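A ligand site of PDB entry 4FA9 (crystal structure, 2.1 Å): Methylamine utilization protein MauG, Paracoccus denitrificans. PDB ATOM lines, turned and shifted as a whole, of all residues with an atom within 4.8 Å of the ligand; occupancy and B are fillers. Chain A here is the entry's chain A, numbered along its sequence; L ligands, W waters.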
ATOM      1  N   PHE A  18      24.387  -1.660  12.545  1.00  0.00           N
ATOM      2  CA  PHE A  18      23.000  -2.025  12.410  1.00  0.00           C
ATOM      3  C   PHE A  18      22.311  -1.896  13.802  1.00  0.00           C
ATOM      4  O   PHE A  18      21.123  -1.499  13.887  1.00  0.00           O
ATOM      5  CB  PHE A  18      22.896  -3.473  11.924  1.00  0.00           C
ATOM      6  CG  PHE A  18      21.481  -3.895  11.658  1.00  0.00           C
ATOM      7  CD1 PHE A  18      20.880  -3.590  10.420  1.00  0.00           C
ATOM      8  CD2 PHE A  18      20.750  -4.597  12.649  1.00  0.00           C
ATOM      9  CE1 PHE A  18      19.580  -3.988  10.154  1.00  0.00           C
ATOM     10  CE2 PHE A  18      19.403  -4.964  12.394  1.00  0.00           C
ATOM     11  CZ  PHE A  18      18.850  -4.671  11.169  1.00  0.00           C
ATOM     12  N   GLN A  29      17.761   5.115  18.913  1.00  0.00           N
ATOM     13  CA  GLN A  29      17.374   3.997  18.031  1.00  0.00           C
ATOM     14  C   GLN A  29      18.379   3.588  16.978  1.00  0.00           C
ATOM     15  O   GLN A  29      19.086   4.415  16.400  1.00  0.00           O
ATOM     16  CB  GLN A  29      15.948   4.150  17.452  1.00  0.00           C
ATOM     17  CG  GLN A  29      15.805   4.907  16.181  1.00  0.00           C
ATOM     18  CD  GLN A  29      14.329   5.067  15.732  1.00  0.00           C
ATOM     19  OE1 GLN A  29      13.343   4.722  16.442  1.00  0.00           O
ATOM     20  NE2 GLN A  29      14.165   5.635  14.571  1.00  0.00           N
ATOM     21  N   SER A  30      18.441   2.277  16.751  1.00  0.00           N
ATOM     22  CA  SER A  30      19.249   1.743  15.719  1.00  0.00           C
ATOM     23  C   SER A  30      18.333   1.123  14.639  1.00  0.00           C
ATOM     24  O   SER A  30      17.075   1.055  14.838  1.00  0.00           O
ATOM     25  CB  SER A  30      20.200   0.723  16.320  1.00  0.00           C
ATOM     26  OG  SER A  30      19.502  -0.446  16.691  1.00  0.00           O
ATOM     27  N   CYS A  31      18.933   0.656  13.536  1.00  0.00           N
ATOM     28  CA  CYS A  31      18.139  -0.110  12.531  1.00  0.00           C
ATOM     29  C   CYS A  31      17.442  -1.269  13.270  1.00  0.00           C
ATOM     30  O   CYS A  31      16.304  -1.550  12.995  1.00  0.00           O
ATOM     31  CB  CYS A  31      19.004  -0.750  11.428  1.00  0.00           C
ATOM     32  SG  CYS A  31      20.262   0.259  10.628  1.00  0.00           S
ATOM     33  N   CYS A  34      13.832  -1.009  14.917  1.00  0.00           N
ATOM     34  CA  CYS A  34      12.666  -1.227  14.107  1.00  0.00           C
ATOM     35  C   CYS A  34      12.732  -2.513  13.400  1.00  0.00           C
ATOM     36  O   CYS A  34      11.706  -3.121  13.107  1.00  0.00           O
ATOM     37  CB  CYS A  34      12.529  -0.131  13.105  1.00  0.00           C
ATOM     38  SG  CYS A  34      12.044   1.342  13.871  1.00  0.00           S
ATOM     39  N   HIS A  35      13.927  -2.943  13.088  1.00  0.00           N
ATOM     40  CA  HIS A  35      14.048  -4.194  12.399  1.00  0.00           C
ATOM     41  C   HIS A  35      14.640  -5.146  13.426  1.00  0.00           C
ATOM     42  O   HIS A  35      15.851  -5.486  13.402  1.00  0.00           O
ATOM     43  CB  HIS A  35      14.870  -4.047  11.157  1.00  0.00           C
ATOM     44  CG  HIS A  35      14.269  -3.109  10.116  1.00  0.00           C
ATOM     45  ND1 HIS A  35      13.286  -3.492   9.225  1.00  0.00           N
ATOM     46  CD2 HIS A  35      14.585  -1.830   9.775  1.00  0.00           C
ATOM     47  CE1 HIS A  35      13.024  -2.500   8.386  1.00  0.00           C
ATOM     48  NE2 HIS A  35      13.795  -1.471   8.714  1.00  0.00           N
ATOM     49  N   ARG A  45       7.500  -3.079  18.839  1.00  0.00           N
ATOM     50  CA  ARG A  45       7.115  -2.006  19.767  1.00  0.00           C
ATOM     51  C   ARG A  45       5.719  -1.491  19.514  1.00  0.00           C
ATOM     52  O   ARG A  45       5.380  -1.120  18.391  1.00  0.00           O
ATOM     53  CB  ARG A  45       8.126  -0.842  19.776  1.00  0.00           C
ATOM     54  CG  ARG A  45       9.555  -1.238  20.210  1.00  0.00           C
ATOM     55  CD  ARG A  45      10.502  -0.090  20.017  1.00  0.00           C
ATOM     56  NE  ARG A  45      10.406   0.359  18.638  1.00  0.00           N
ATOM     57  CZ  ARG A  45      10.563   1.608  18.209  1.00  0.00           C
ATOM     58  NH1 ARG A  45      10.884   2.585  19.062  1.00  0.00           N
ATOM     59  NH2 ARG A  45      10.398   1.862  16.903  1.00  0.00           N
ATOM     60  N   SER A  54       5.701   2.285  13.030  1.00  0.00           N
ATOM     61  CA  SER A  54       6.760   2.336  14.022  1.00  0.00           C
ATOM     62  C   SER A  54       6.995   3.777  14.409  1.00  0.00           C
ATOM     63  O   SER A  54       6.722   4.707  13.622  1.00  0.00           O
ATOM     64  CB  SER A  54       8.047   1.813  13.362  1.00  0.00           C
ATOM     65  OG  SER A  54       7.982   0.412  13.156  1.00  0.00           O
ATOM     66  N   VAL A  55       7.570   3.951  15.621  1.00  0.00           N
ATOM     67  CA  VAL A  55       7.876   5.263  16.163  1.00  0.00           C
ATOM     68  C   VAL A  55       9.326   5.668  15.948  1.00  0.00           C
ATOM     69  O   VAL A  55      10.227   4.883  16.254  1.00  0.00           O
ATOM     70  CB  VAL A  55       7.467   5.266  17.645  1.00  0.00           C
ATOM     71  CG1 VAL A  55       7.662   6.639  18.289  1.00  0.00           C
ATOM     72  CG2 VAL A  55       5.992   4.836  17.680  1.00  0.00           C
ATOM     73  N   GLY A  56       9.575   6.884  15.459  1.00  0.00           N
ATOM     74  CA  GLY A  56      10.952   7.335  15.231  1.00  0.00           C
ATOM     75  C   GLY A  56      11.765   7.687  16.495  1.00  0.00           C
ATOM     76  O   GLY A  56      11.272   7.553  17.642  1.00  0.00           O
ATOM     77  N   ARG A  65       3.776   3.620   7.016  1.00  0.00           N
ATOM     78  CA  ARG A  65       3.902   2.274   6.481  1.00  0.00           C
ATOM     79  C   ARG A  65       4.459   1.360   7.518  1.00  0.00           C
ATOM     80  O   ARG A  65       5.190   1.817   8.431  1.00  0.00           O
ATOM     81  CB  ARG A  65       4.784   2.324   5.255  1.00  0.00           C
ATOM     82  CG  ARG A  65       4.022   2.921   4.089  1.00  0.00           C
ATOM     83  CD  ARG A  65       4.942   3.082   2.978  1.00  0.00           C
ATOM     84  NE  ARG A  65       4.269   3.613   1.798  1.00  0.00           N
ATOM     85  CZ  ARG A  65       4.924   4.031   0.720  1.00  0.00           C
ATOM     86  NH1 ARG A  65       6.254   3.937   0.672  1.00  0.00           N
ATOM     87  NH2 ARG A  65       4.269   4.469  -0.337  1.00  0.00           N
ATOM     88  N   ASN A  66       4.064   0.089   7.431  1.00  0.00           N
ATOM     89  CA  ASN A  66       4.484  -0.996   8.345  1.00  0.00           C
ATOM     90  C   ASN A  66       5.948  -1.300   8.023  1.00  0.00           C
ATOM     91  O   ASN A  66       6.357  -1.303   6.836  1.00  0.00           O
ATOM     92  CB  ASN A  66       3.583  -2.200   8.057  1.00  0.00           C
ATOM     93  CG  ASN A  66       3.891  -3.433   8.919  1.00  0.00           C
ATOM     94  OD1 ASN A  66       4.336  -4.469   8.375  1.00  0.00           O
ATOM     95  ND2 ASN A  66       3.611  -3.361  10.261  1.00  0.00           N
ATOM     96  N   THR A  67       6.733  -1.499   9.061  1.00  0.00           N
ATOM     97  CA  THR A  67       8.121  -1.829   8.912  1.00  0.00           C
ATOM     98  C   THR A  67       8.216  -3.271   8.449  1.00  0.00           C
ATOM     99  O   THR A  67       7.817  -4.176   9.176  1.00  0.00           O
ATOM    100  CB  THR A  67       8.813  -1.663  10.243  1.00  0.00           C
ATOM    101  OG1 THR A  67       8.783  -0.278  10.640  1.00  0.00           O
ATOM    102  CG2 THR A  67      10.254  -2.161  10.161  1.00  0.00           C
ATOM    103  N   PRO A  68       8.743  -3.492   7.228  1.00  0.00           N
ATOM    104  CA  PRO A  68       8.892  -4.828   6.647  1.00  0.00           C
ATOM    105  C   PRO A  68      10.141  -5.603   7.163  1.00  0.00           C
ATOM    106  O   PRO A  68      11.164  -5.026   7.612  1.00  0.00           O
ATOM    107  CB  PRO A  68       9.035  -4.525   5.117  1.00  0.00           C
ATOM    108  CG  PRO A  68       9.799  -3.158   5.141  1.00  0.00           C
ATOM    109  CD  PRO A  68       9.458  -2.465   6.456  1.00  0.00           C
ATOM    110  N   THR A  69      10.079  -6.926   7.096  1.00  0.00           N
ATOM    111  CA  THR A  69      11.267  -7.712   7.390  1.00  0.00           C
ATOM    112  C   THR A  69      12.424  -7.331   6.459  1.00  0.00           C
ATOM    113  O   THR A  69      12.218  -6.911   5.308  1.00  0.00           O
ATOM    114  CB  THR A  69      11.009  -9.202   7.201  1.00  0.00           C
ATOM    115  OG1 THR A  69      12.180  -9.877   7.582  1.00  0.00           O
ATOM    116  CG2 THR A  69      10.689  -9.520   5.742  1.00  0.00           C
ATOM    117  N   LEU A  70      13.631  -7.488   6.960  1.00  0.00           N
ATOM    118  CA  LEU A  70      14.812  -7.371   6.117  1.00  0.00           C
ATOM    119  C   LEU A  70      15.243  -8.802   5.643  1.00  0.00           C
ATOM    120  O   LEU A  70      16.113  -8.919   4.788  1.00  0.00           O
ATOM    121  CB  LEU A  70      15.955  -6.702   6.875  1.00  0.00           C
ATOM    122  CG  LEU A  70      15.685  -5.302   7.458  1.00  0.00           C
ATOM    123  CD1 LEU A  70      16.967  -4.744   8.040  1.00  0.00           C
ATOM    124  CD2 LEU A  70      15.124  -4.306   6.396  1.00  0.00           C
ATOM    125  N   ALA A  73      15.419  -9.679   1.792  1.00  0.00           N
ATOM    126  CA  ALA A  73      15.437  -8.452   0.984  1.00  0.00           C
ATOM    127  C   ALA A  73      16.621  -8.417   0.045  1.00  0.00           C
ATOM    128  O   ALA A  73      16.520  -7.830  -0.994  1.00  0.00           O
ATOM    129  CB  ALA A  73      15.397  -7.192   1.842  1.00  0.00           C
ATOM    130  N   GLN A  91      13.623  -1.391  -3.323  1.00  0.00           N
ATOM    131  CA  GLN A  91      13.384  -1.535  -1.868  1.00  0.00           C
ATOM    132  C   GLN A  91      12.433  -0.457  -1.392  1.00  0.00           C
ATOM    133  O   GLN A  91      12.235   0.560  -2.079  1.00  0.00           O
ATOM    134  CB  GLN A  91      14.668  -1.466  -1.042  1.00  0.00           C
ATOM    135  CG  GLN A  91      15.709  -2.546  -1.388  1.00  0.00           C
ATOM    136  CD  GLN A  91      15.314  -3.955  -0.987  1.00  0.00           C
ATOM    137  OE1 GLN A  91      15.897  -4.961  -1.497  1.00  0.00           O
ATOM    138  NE2 GLN A  91      14.371  -4.076  -0.085  1.00  0.00           N
ATOM    139  N   PHE A  92      11.839  -0.702  -0.230  1.00  0.00           N
ATOM    140  CA  PHE A  92      10.624   0.026   0.257  1.00  0.00           C
ATOM    141  C   PHE A  92       9.353  -0.513  -0.453  1.00  0.00           C
ATOM    142  O   PHE A  92       9.417  -1.056  -1.561  1.00  0.00           O
ATOM    143  CB  PHE A  92      10.672   1.532   0.039  1.00  0.00           C
ATOM    144  CG  PHE A  92      11.674   2.274   0.883  1.00  0.00           C
ATOM    145  CD1 PHE A  92      11.649   2.195   2.258  1.00  0.00           C
ATOM    146  CD2 PHE A  92      12.608   3.106   0.281  1.00  0.00           C
ATOM    147  CE1 PHE A  92      12.568   2.904   3.053  1.00  0.00           C
ATOM    148  CE2 PHE A  92      13.524   3.789   1.087  1.00  0.00           C
ATOM    149  CZ  PHE A  92      13.481   3.715   2.451  1.00  0.00           C
ATOM    150  N   TRP A  93       8.195  -0.306   0.180  1.00  0.00           N
ATOM    151  CA  TRP A  93       6.958  -0.851  -0.349  1.00  0.00           C
ATOM    152  C   TRP A  93       6.639  -0.208  -1.659  1.00  0.00           C
ATOM    153  O   TRP A  93       5.908  -0.787  -2.465  1.00  0.00           O
ATOM    154  CB  TRP A  93       5.838  -0.547   0.593  1.00  0.00           C
ATOM    155  CG  TRP A  93       5.834  -1.276   1.802  1.00  0.00           C
ATOM    156  CD1 TRP A  93       6.260  -0.846   3.007  1.00  0.00           C
ATOM    157  CD2 TRP A  93       5.297  -2.569   1.992  1.00  0.00           C
ATOM    158  NE1 TRP A  93       6.004  -1.805   3.980  1.00  0.00           N
ATOM    159  CE2 TRP A  93       5.418  -2.881   3.369  1.00  0.00           C
ATOM    160  CE3 TRP A  93       4.655  -3.494   1.154  1.00  0.00           C
ATOM    161  CZ2 TRP A  93       4.946  -4.105   3.910  1.00  0.00           C
ATOM    162  CZ3 TRP A  93       4.208  -4.733   1.719  1.00  0.00           C
ATOM    163  CH2 TRP A  93       4.335  -5.001   3.058  1.00  0.00           C
ATOM    164  N   ASP A  94       7.179   0.980  -1.891  1.00  0.00           N
ATOM    165  CA  ASP A  94       6.874   1.666  -3.154  1.00  0.00           C
ATOM    166  C   ASP A  94       8.061   1.679  -4.090  1.00  0.00           C
ATOM    167  O   ASP A  94       8.077   2.419  -5.084  1.00  0.00           O
ATOM    168  CB  ASP A  94       6.380   3.093  -2.889  1.00  0.00           C
ATOM    169  CG  ASP A  94       7.384   3.922  -2.142  1.00  0.00           C
ATOM    170  OD1 ASP A  94       7.013   5.024  -1.752  1.00  0.00           O
ATOM    171  OD2 ASP A  94       8.535   3.479  -1.904  1.00  0.00           O
ATOM    172  N   ARG A  96      10.930   2.943  -4.052  1.00  0.00           N
ATOM    173  CA  ARG A  96      11.542   4.214  -4.349  1.00  0.00           C
ATOM    174  C   ARG A  96      13.081   4.201  -4.151  1.00  0.00           C
ATOM    175  O   ARG A  96      13.774   5.102  -4.617  1.00  0.00           O
ATOM    176  CB  ARG A  96      10.829   5.310  -3.573  1.00  0.00           C
ATOM    177  CG  ARG A  96      11.150   5.298  -2.052  1.00  0.00           C
ATOM    178  CD  ARG A  96      10.580   6.543  -1.323  1.00  0.00           C
ATOM    179  NE  ARG A  96      10.876   6.534   0.115  1.00  0.00           N
ATOM    180  CZ  ARG A  96      10.279   5.746   1.020  1.00  0.00           C
ATOM    181  NH1 ARG A  96      10.612   5.809   2.296  1.00  0.00           N
ATOM    182  NH2 ARG A  96       9.357   4.864   0.652  1.00  0.00           N
ATOM    183  N   LEU A 100      19.661  -2.141  -1.855  1.00  0.00           N
ATOM    184  CA  LEU A 100      19.821  -2.006  -0.395  1.00  0.00           C
ATOM    185  C   LEU A 100      20.782  -0.896  -0.049  1.00  0.00           C
ATOM    186  O   LEU A 100      20.603  -0.237   0.974  1.00  0.00           O
ATOM    187  CB  LEU A 100      20.331  -3.297   0.229  1.00  0.00           C
ATOM    188  CG  LEU A 100      19.352  -4.426   0.235  1.00  0.00           C
ATOM    189  CD1 LEU A 100      20.102  -5.719   0.545  1.00  0.00           C
ATOM    190  CD2 LEU A 100      18.203  -4.135   1.230  1.00  0.00           C
ATOM    191  N   GLN A 103      18.902   2.341  -0.316  1.00  0.00           N
ATOM    192  CA  GLN A 103      17.932   2.383   0.789  1.00  0.00           C
ATOM    193  C   GLN A 103      18.517   2.765   2.189  1.00  0.00           C
ATOM    194  O   GLN A 103      17.806   3.442   2.965  1.00  0.00           O
ATOM    195  CB  GLN A 103      17.237   1.019   0.935  1.00  0.00           C
ATOM    196  CG  GLN A 103      15.952   1.106   1.803  1.00  0.00           C
ATOM    197  CD  GLN A 103      16.308   1.143   3.281  1.00  0.00           C
ATOM    198  OE1 GLN A 103      17.441   0.747   3.707  1.00  0.00           O
ATOM    199  NE2 GLN A 103      15.361   1.616   4.089  1.00  0.00           N
ATOM    200  N   ALA A 104      19.765   2.359   2.490  1.00  0.00           N
ATOM    201  CA  ALA A 104      20.297   2.305   3.897  1.00  0.00           C
ATOM    202  C   ALA A 104      20.448   3.662   4.566  1.00  0.00           C
ATOM    203  O   ALA A 104      20.202   3.813   5.762  1.00  0.00           O
ATOM    204  CB  ALA A 104      21.690   1.493   3.971  1.00  0.00           C
ATOM    205  N   PRO A 107      16.630   5.808   6.249  1.00  0.00           N
ATOM    206  CA  PRO A 107      16.174   5.937   7.658  1.00  0.00           C
ATOM    207  C   PRO A 107      17.029   6.837   8.592  1.00  0.00           C
ATOM    208  O   PRO A 107      16.485   7.437   9.566  1.00  0.00           O
ATOM    209  CB  PRO A 107      16.182   4.478   8.198  1.00  0.00           C
ATOM    210  CG  PRO A 107      16.605   3.572   7.025  1.00  0.00           C
ATOM    211  CD  PRO A 107      16.535   4.421   5.762  1.00  0.00           C
ATOM    212  N   MET A 108      18.339   6.873   8.347  1.00  0.00           N
ATOM    213  CA  MET A 108      19.238   7.738   9.105  1.00  0.00           C
ATOM    214  C   MET A 108      18.864   9.217   9.108  1.00  0.00           C
ATOM    215  O   MET A 108      18.976   9.885  10.141  1.00  0.00           O
ATOM    216  CB  MET A 108      20.667   7.629   8.610  1.00  0.00           C
ATOM    217  CG  MET A 108      21.358   6.354   9.089  1.00  0.00           C
ATOM    218  SD  MET A 108      22.969   6.137   8.275  1.00  0.00           S
ATOM    219  CE  MET A 108      22.882   4.373   7.951  1.00  0.00           C
ATOM    220  N   GLU A 113      12.039   8.964  11.351  1.00  0.00           N
ATOM    221  CA  GLU A 113      12.759   7.790  11.852  1.00  0.00           C
ATOM    222  C   GLU A 113      13.976   8.162  12.702  1.00  0.00           C
ATOM    223  O   GLU A 113      13.844   8.686  13.846  1.00  0.00           O
ATOM    224  CB  GLU A 113      13.099   6.842  10.679  1.00  0.00           C
ATOM    225  CG  GLU A 113      11.788   6.342  10.015  1.00  0.00           C
ATOM    226  CD  GLU A 113      11.998   5.703   8.609  1.00  0.00           C
ATOM    227  OE1 GLU A 113      13.001   6.064   7.920  1.00  0.00           O
ATOM    228  OE2 GLU A 113      11.163   4.848   8.209  1.00  0.00           O
ATOM    229  N   MET A 114      15.161   7.889  12.186  1.00  0.00           N
ATOM    230  CA  MET A 114      16.339   8.114  12.995  1.00  0.00           C
ATOM    231  C   MET A 114      16.698   9.577  13.173  1.00  0.00           C
ATOM    232  O   MET A 114      17.241   9.956  14.234  1.00  0.00           O
ATOM    233  CB  MET A 114      17.526   7.248  12.560  1.00  0.00           C
ATOM    234  CG  MET A 114      17.156   5.763  12.589  1.00  0.00           C
ATOM    235  SD  MET A 114      18.340   4.688  11.757  1.00  0.00           S
ATOM    236  CE  MET A 114      19.389   4.314  13.168  1.00  0.00           C
ATOM    237  N   LEU A 159      26.054  -1.634   5.763  1.00  0.00           N
ATOM    238  CA  LEU A 159      24.719  -2.136   6.072  1.00  0.00           C
ATOM    239  C   LEU A 159      24.156  -3.072   4.964  1.00  0.00           C
ATOM    240  O   LEU A 159      23.609  -4.142   5.268  1.00  0.00           O
ATOM    241  CB  LEU A 159      23.771  -0.945   6.317  1.00  0.00           C
ATOM    242  CG  LEU A 159      24.174  -0.354   7.689  1.00  0.00           C
ATOM    243  CD1 LEU A 159      23.809   1.105   7.768  1.00  0.00           C
ATOM    244  CD2 LEU A 159      23.627  -1.124   8.934  1.00  0.00           C
ATOM    245  N   GLN A 163      23.241  -6.921   5.238  1.00  0.00           N
ATOM    246  CA  GLN A 163      21.931  -7.518   4.857  1.00  0.00           C
ATOM    247  C   GLN A 163      22.002  -8.622   3.797  1.00  0.00           C
ATOM    248  O   GLN A 163      21.001  -9.345   3.580  1.00  0.00           O
ATOM    249  CB  GLN A 163      20.905  -6.462   4.464  1.00  0.00           C
ATOM    250  CG  GLN A 163      20.529  -5.526   5.605  1.00  0.00           C
ATOM    251  CD  GLN A 163      19.827  -4.342   5.095  1.00  0.00           C
ATOM    252  OE1 GLN A 163      20.485  -3.327   4.719  1.00  0.00           O
ATOM    253  NE2 GLN A 163      18.507  -4.449   4.974  1.00  0.00           N
ATOM    254  N   LYS A 265       4.984  -3.029  -3.870  1.00  0.00           N
ATOM    255  CA  LYS A 265       5.848  -4.187  -4.156  1.00  0.00           C
ATOM    256  C   LYS A 265       5.299  -5.439  -3.550  1.00  0.00           C
ATOM    257  O   LYS A 265       4.907  -5.439  -2.366  1.00  0.00           O
ATOM    258  CB  LYS A 265       7.276  -3.957  -3.677  1.00  0.00           C
ATOM    259  CG  LYS A 265       8.196  -5.174  -3.741  1.00  0.00           C
ATOM    260  CD  LYS A 265       9.663  -4.705  -3.520  1.00  0.00           C
ATOM    261  CE  LYS A 265      10.025  -4.353  -2.012  1.00  0.00           C
ATOM    262  NZ  LYS A 265       9.634  -5.258  -0.784  1.00  0.00           N
HETATM  263 FE1  LIG L   1      13.941   0.317   7.739  1.00  0.00          FE
HETATM  264  C1  LIG L   1      11.945  -0.384   5.113  1.00  0.00           C
HETATM  265  C2  LIG L   1      16.643  -1.144   6.136  1.00  0.00           C
HETATM  266  C3  LIG L   1      16.079   1.695  10.043  1.00  0.00           C
HETATM  267  C4  LIG L   1      11.264   1.276   9.609  1.00  0.00           C
HETATM  268  N1  LIG L   1      14.233  -0.650   5.945  1.00  0.00           N
HETATM  269  C5  LIG L   1      13.335  -0.853   4.984  1.00  0.00           C
HETATM  270  C6  LIG L   1      13.866  -1.600   3.800  1.00  0.00           C
HETATM  271  C7  LIG L   1      15.204  -1.812   4.097  1.00  0.00           C
HETATM  272  C8  LIG L   1      15.369  -1.152   5.431  1.00  0.00           C
HETATM  273  C9  LIG L   1      16.271  -2.505   3.268  1.00  0.00           C
HETATM  274  C10 LIG L   1      13.152  -2.078   2.565  1.00  0.00           C
HETATM  275  C11 LIG L   1      12.651  -3.505   2.842  1.00  0.00           C
HETATM  276  C12 LIG L   1      11.645  -3.847   1.729  1.00  0.00           C
HETATM  277  O1  LIG L   1      11.143  -4.984   1.667  1.00  0.00           O
HETATM  278  O2  LIG L   1      11.287  -2.975   0.904  1.00  0.00           O
HETATM  279  N2  LIG L   1      16.002   0.265   8.031  1.00  0.00           N
HETATM  280  C13 LIG L   1      16.946  -0.341   7.323  1.00  0.00           C
HETATM  281  C14 LIG L   1      18.343  -0.087   7.767  1.00  0.00           C
HETATM  282  C15 LIG L   1      18.171   0.728   8.893  1.00  0.00           C
HETATM  283  C16 LIG L   1      16.705   0.892   8.990  1.00  0.00           C
HETATM  284  C17 LIG L   1      19.585  -0.677   7.105  1.00  0.00           C
HETATM  285  C18 LIG L   1      19.175   1.372   9.834  1.00  0.00           C
HETATM  286  C19 LIG L   1      20.054   2.359   9.049  1.00  0.00           C
HETATM  287  N3  LIG L   1      13.670   1.333   9.521  1.00  0.00           N
HETATM  288  C20 LIG L   1      14.635   1.741  10.345  1.00  0.00           C
HETATM  289  C21 LIG L   1      14.143   2.274  11.628  1.00  0.00           C
HETATM  290  C22 LIG L   1      12.750   2.178  11.554  1.00  0.00           C
HETATM  291  C23 LIG L   1      12.543   1.581  10.198  1.00  0.00           C
HETATM  292  C24 LIG L   1      15.051   2.800  12.704  1.00  0.00           C
HETATM  293  C25 LIG L   1      11.645   2.524  12.556  1.00  0.00           C
HETATM  294  C26 LIG L   1      11.709   3.914  13.062  1.00  0.00           C
HETATM  295  N4  LIG L   1      11.892   0.388   7.439  1.00  0.00           N
HETATM  296  C27 LIG L   1      10.973   0.968   8.176  1.00  0.00           C
HETATM  297  C28 LIG L   1       9.698   1.228   7.495  1.00  0.00           C
HETATM  298  C29 LIG L   1       9.902   0.756   6.204  1.00  0.00           C
HETATM  299  C30 LIG L   1      11.301   0.281   6.252  1.00  0.00           C
HETATM  300  C31 LIG L   1       8.475   1.891   8.062  1.00  0.00           C
HETATM  301  C32 LIG L   1       9.020   0.778   5.001  1.00  0.00           C
HETATM  302  C33 LIG L   1       8.974   2.275   4.644  1.00  0.00           C
HETATM  303  C34 LIG L   1       8.420   2.470   3.271  1.00  0.00           C
HETATM  304  O3  LIG L   1       8.310   3.651   2.857  1.00  0.00           O
HETATM  305  O4  LIG L   1       8.082   1.489   2.578  1.00  0.00           O
HETATM  306  O   HOH W   1       8.636  -3.631   1.834  1.00  0.00           O
HETATM  307  O   HOH W   2      11.666  -7.103   2.868  1.00  0.00           O
HETATM  308  O   HOH W   3      12.528   3.541   6.253  1.00  0.00           O
HETATM  309  O   HOH W   4       6.514   3.162  10.422  1.00  0.00           O
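Water W2 lies within hydrogen-bond range of O1 of the ligand and O of Thr 69.
Water W1 bridges an oxygen (O1) of the ligand (2.9 Å) and the side-chain amino group (NZ) of Lys 265 (3.2 Å).
Water W4 bridges the backbone carbonyl oxygen (O) of Arg 65 (2.7 Å) and the backbone NH (N) of Ser 54 (2.9 Å).
The side-chain amide nitrogen of Gln 103 lies close to a nitrogen (N1) of the ligand (3.1 Å).
Gln 29 touches the ligand (NE2 to C26, 3.4 Å).
O of Ser 30 touches C24 of the ligand, 3.4 Å away.
CB of Ser 54 touches C25 of the ligand, 3.8 Å away.
Val 55 touches the ligand (O to C26, 3.7 Å).
O of Asn 66 touches C32 of the ligand, 3.8 Å away.
OG1 of Thr 67 touches C4 of the ligand (3.1 Å).
Pro 68 touches the ligand.
CD2 of Leu 70 touches C8 of the ligand, at 3.3 Å.
CD2 of Leu 100 touches C9 of the ligand, 3.2 Å away.
Ala 104 touches the ligand.
Pro 107 touches the ligand.
Met 108 touches the ligand (CE to C19, 3.6 Å).
Glu 113 touches the ligand (OE2 to C4, 3.8 Å).
Met 114 touches the ligand.
NE2 of Gln 163 touches C9 of the ligand, at 3.4 Å.
Hydrophobic or aromatic side chains that line the ligand: His 35, Pro 68, Leu 70, Phe 92, Trp 93, Leu 100, Pro 107, Met 108 and Met 114.
25 residues have an atom within 4 Å of the ligand: Gln 29, Ser 30, Cys 31, Cys 34, His 35, Ser 54, Val 55, Arg 65, Asn 66, Thr 67, Pro 68, Leu 70, Gln 91, Phe 92, Trp 93, Arg 96, Leu 100, Gln 103, Ala 104, Pro 107, Met 108, Glu 113, Met 114, Gln 163 and Lys 265.
O of Val 55 lies within hydrogen-bond range of NH2 of Arg 45 (3.1 Å).
The side-chain sulfur of Cys 34 sits at hydrogen-bond distance from the guanidinium group of Arg 45, at 3.5 Å.
O of Asn 66 lies within hydrogen-bond range of NE1 of Trp 93 (2.9 Å).
OD2 of Asp 94 lies within salt-bridge range of NH2 of Arg 96, 3.0 Å away.
The backbone NH of Cys 31 sits at hydrogen-bond distance from the backbone carbonyl oxygen of Phe 18 (3.1 Å).
NH1 of Arg 65 lies within salt-bridge range of OD1 of Asp 94 (2.8 Å).
The backbone NH (N) of Met 114 lies within hydrogen-bond range of the backbone carbonyl oxygen (O) of Pro 107, 3.0 Å away.
NE2 of Gln 29 sits close to O of Glu 113, at 3.2 Å.
The side-chain sulfur of Cys 34 is bonded to a carbon (C25) of the ligand (1.8 Å).
An oxygen (O2) of the ligand lies within hydrogen-bond range of the backbone NH (N) of Phe 92, at 2.6 Å.
SG of Cys 31 is bonded to C18 of the ligand.
N of Trp 93 sits close to O4 of the ligand.
NZ of Lys 265 is in salt-bridge range of O1 of the ligand, at 2.9 Å.
An oxygen (O2) of the ligand sits close to the side-chain amide nitrogen (NE2) of Gln 91, 3.4 Å away.
NE2 of His 35 binds FE1 of the ligand (2.0 Å).
An oxygen (O3) of the ligand is in salt-bridge range of the guanidinium group (NH2) of Arg 96 (2.7 Å).
The guanidinium group (NH1) of Arg 65 lies within salt-bridge range of an oxygen (O3) of the ligand (3.0 Å).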
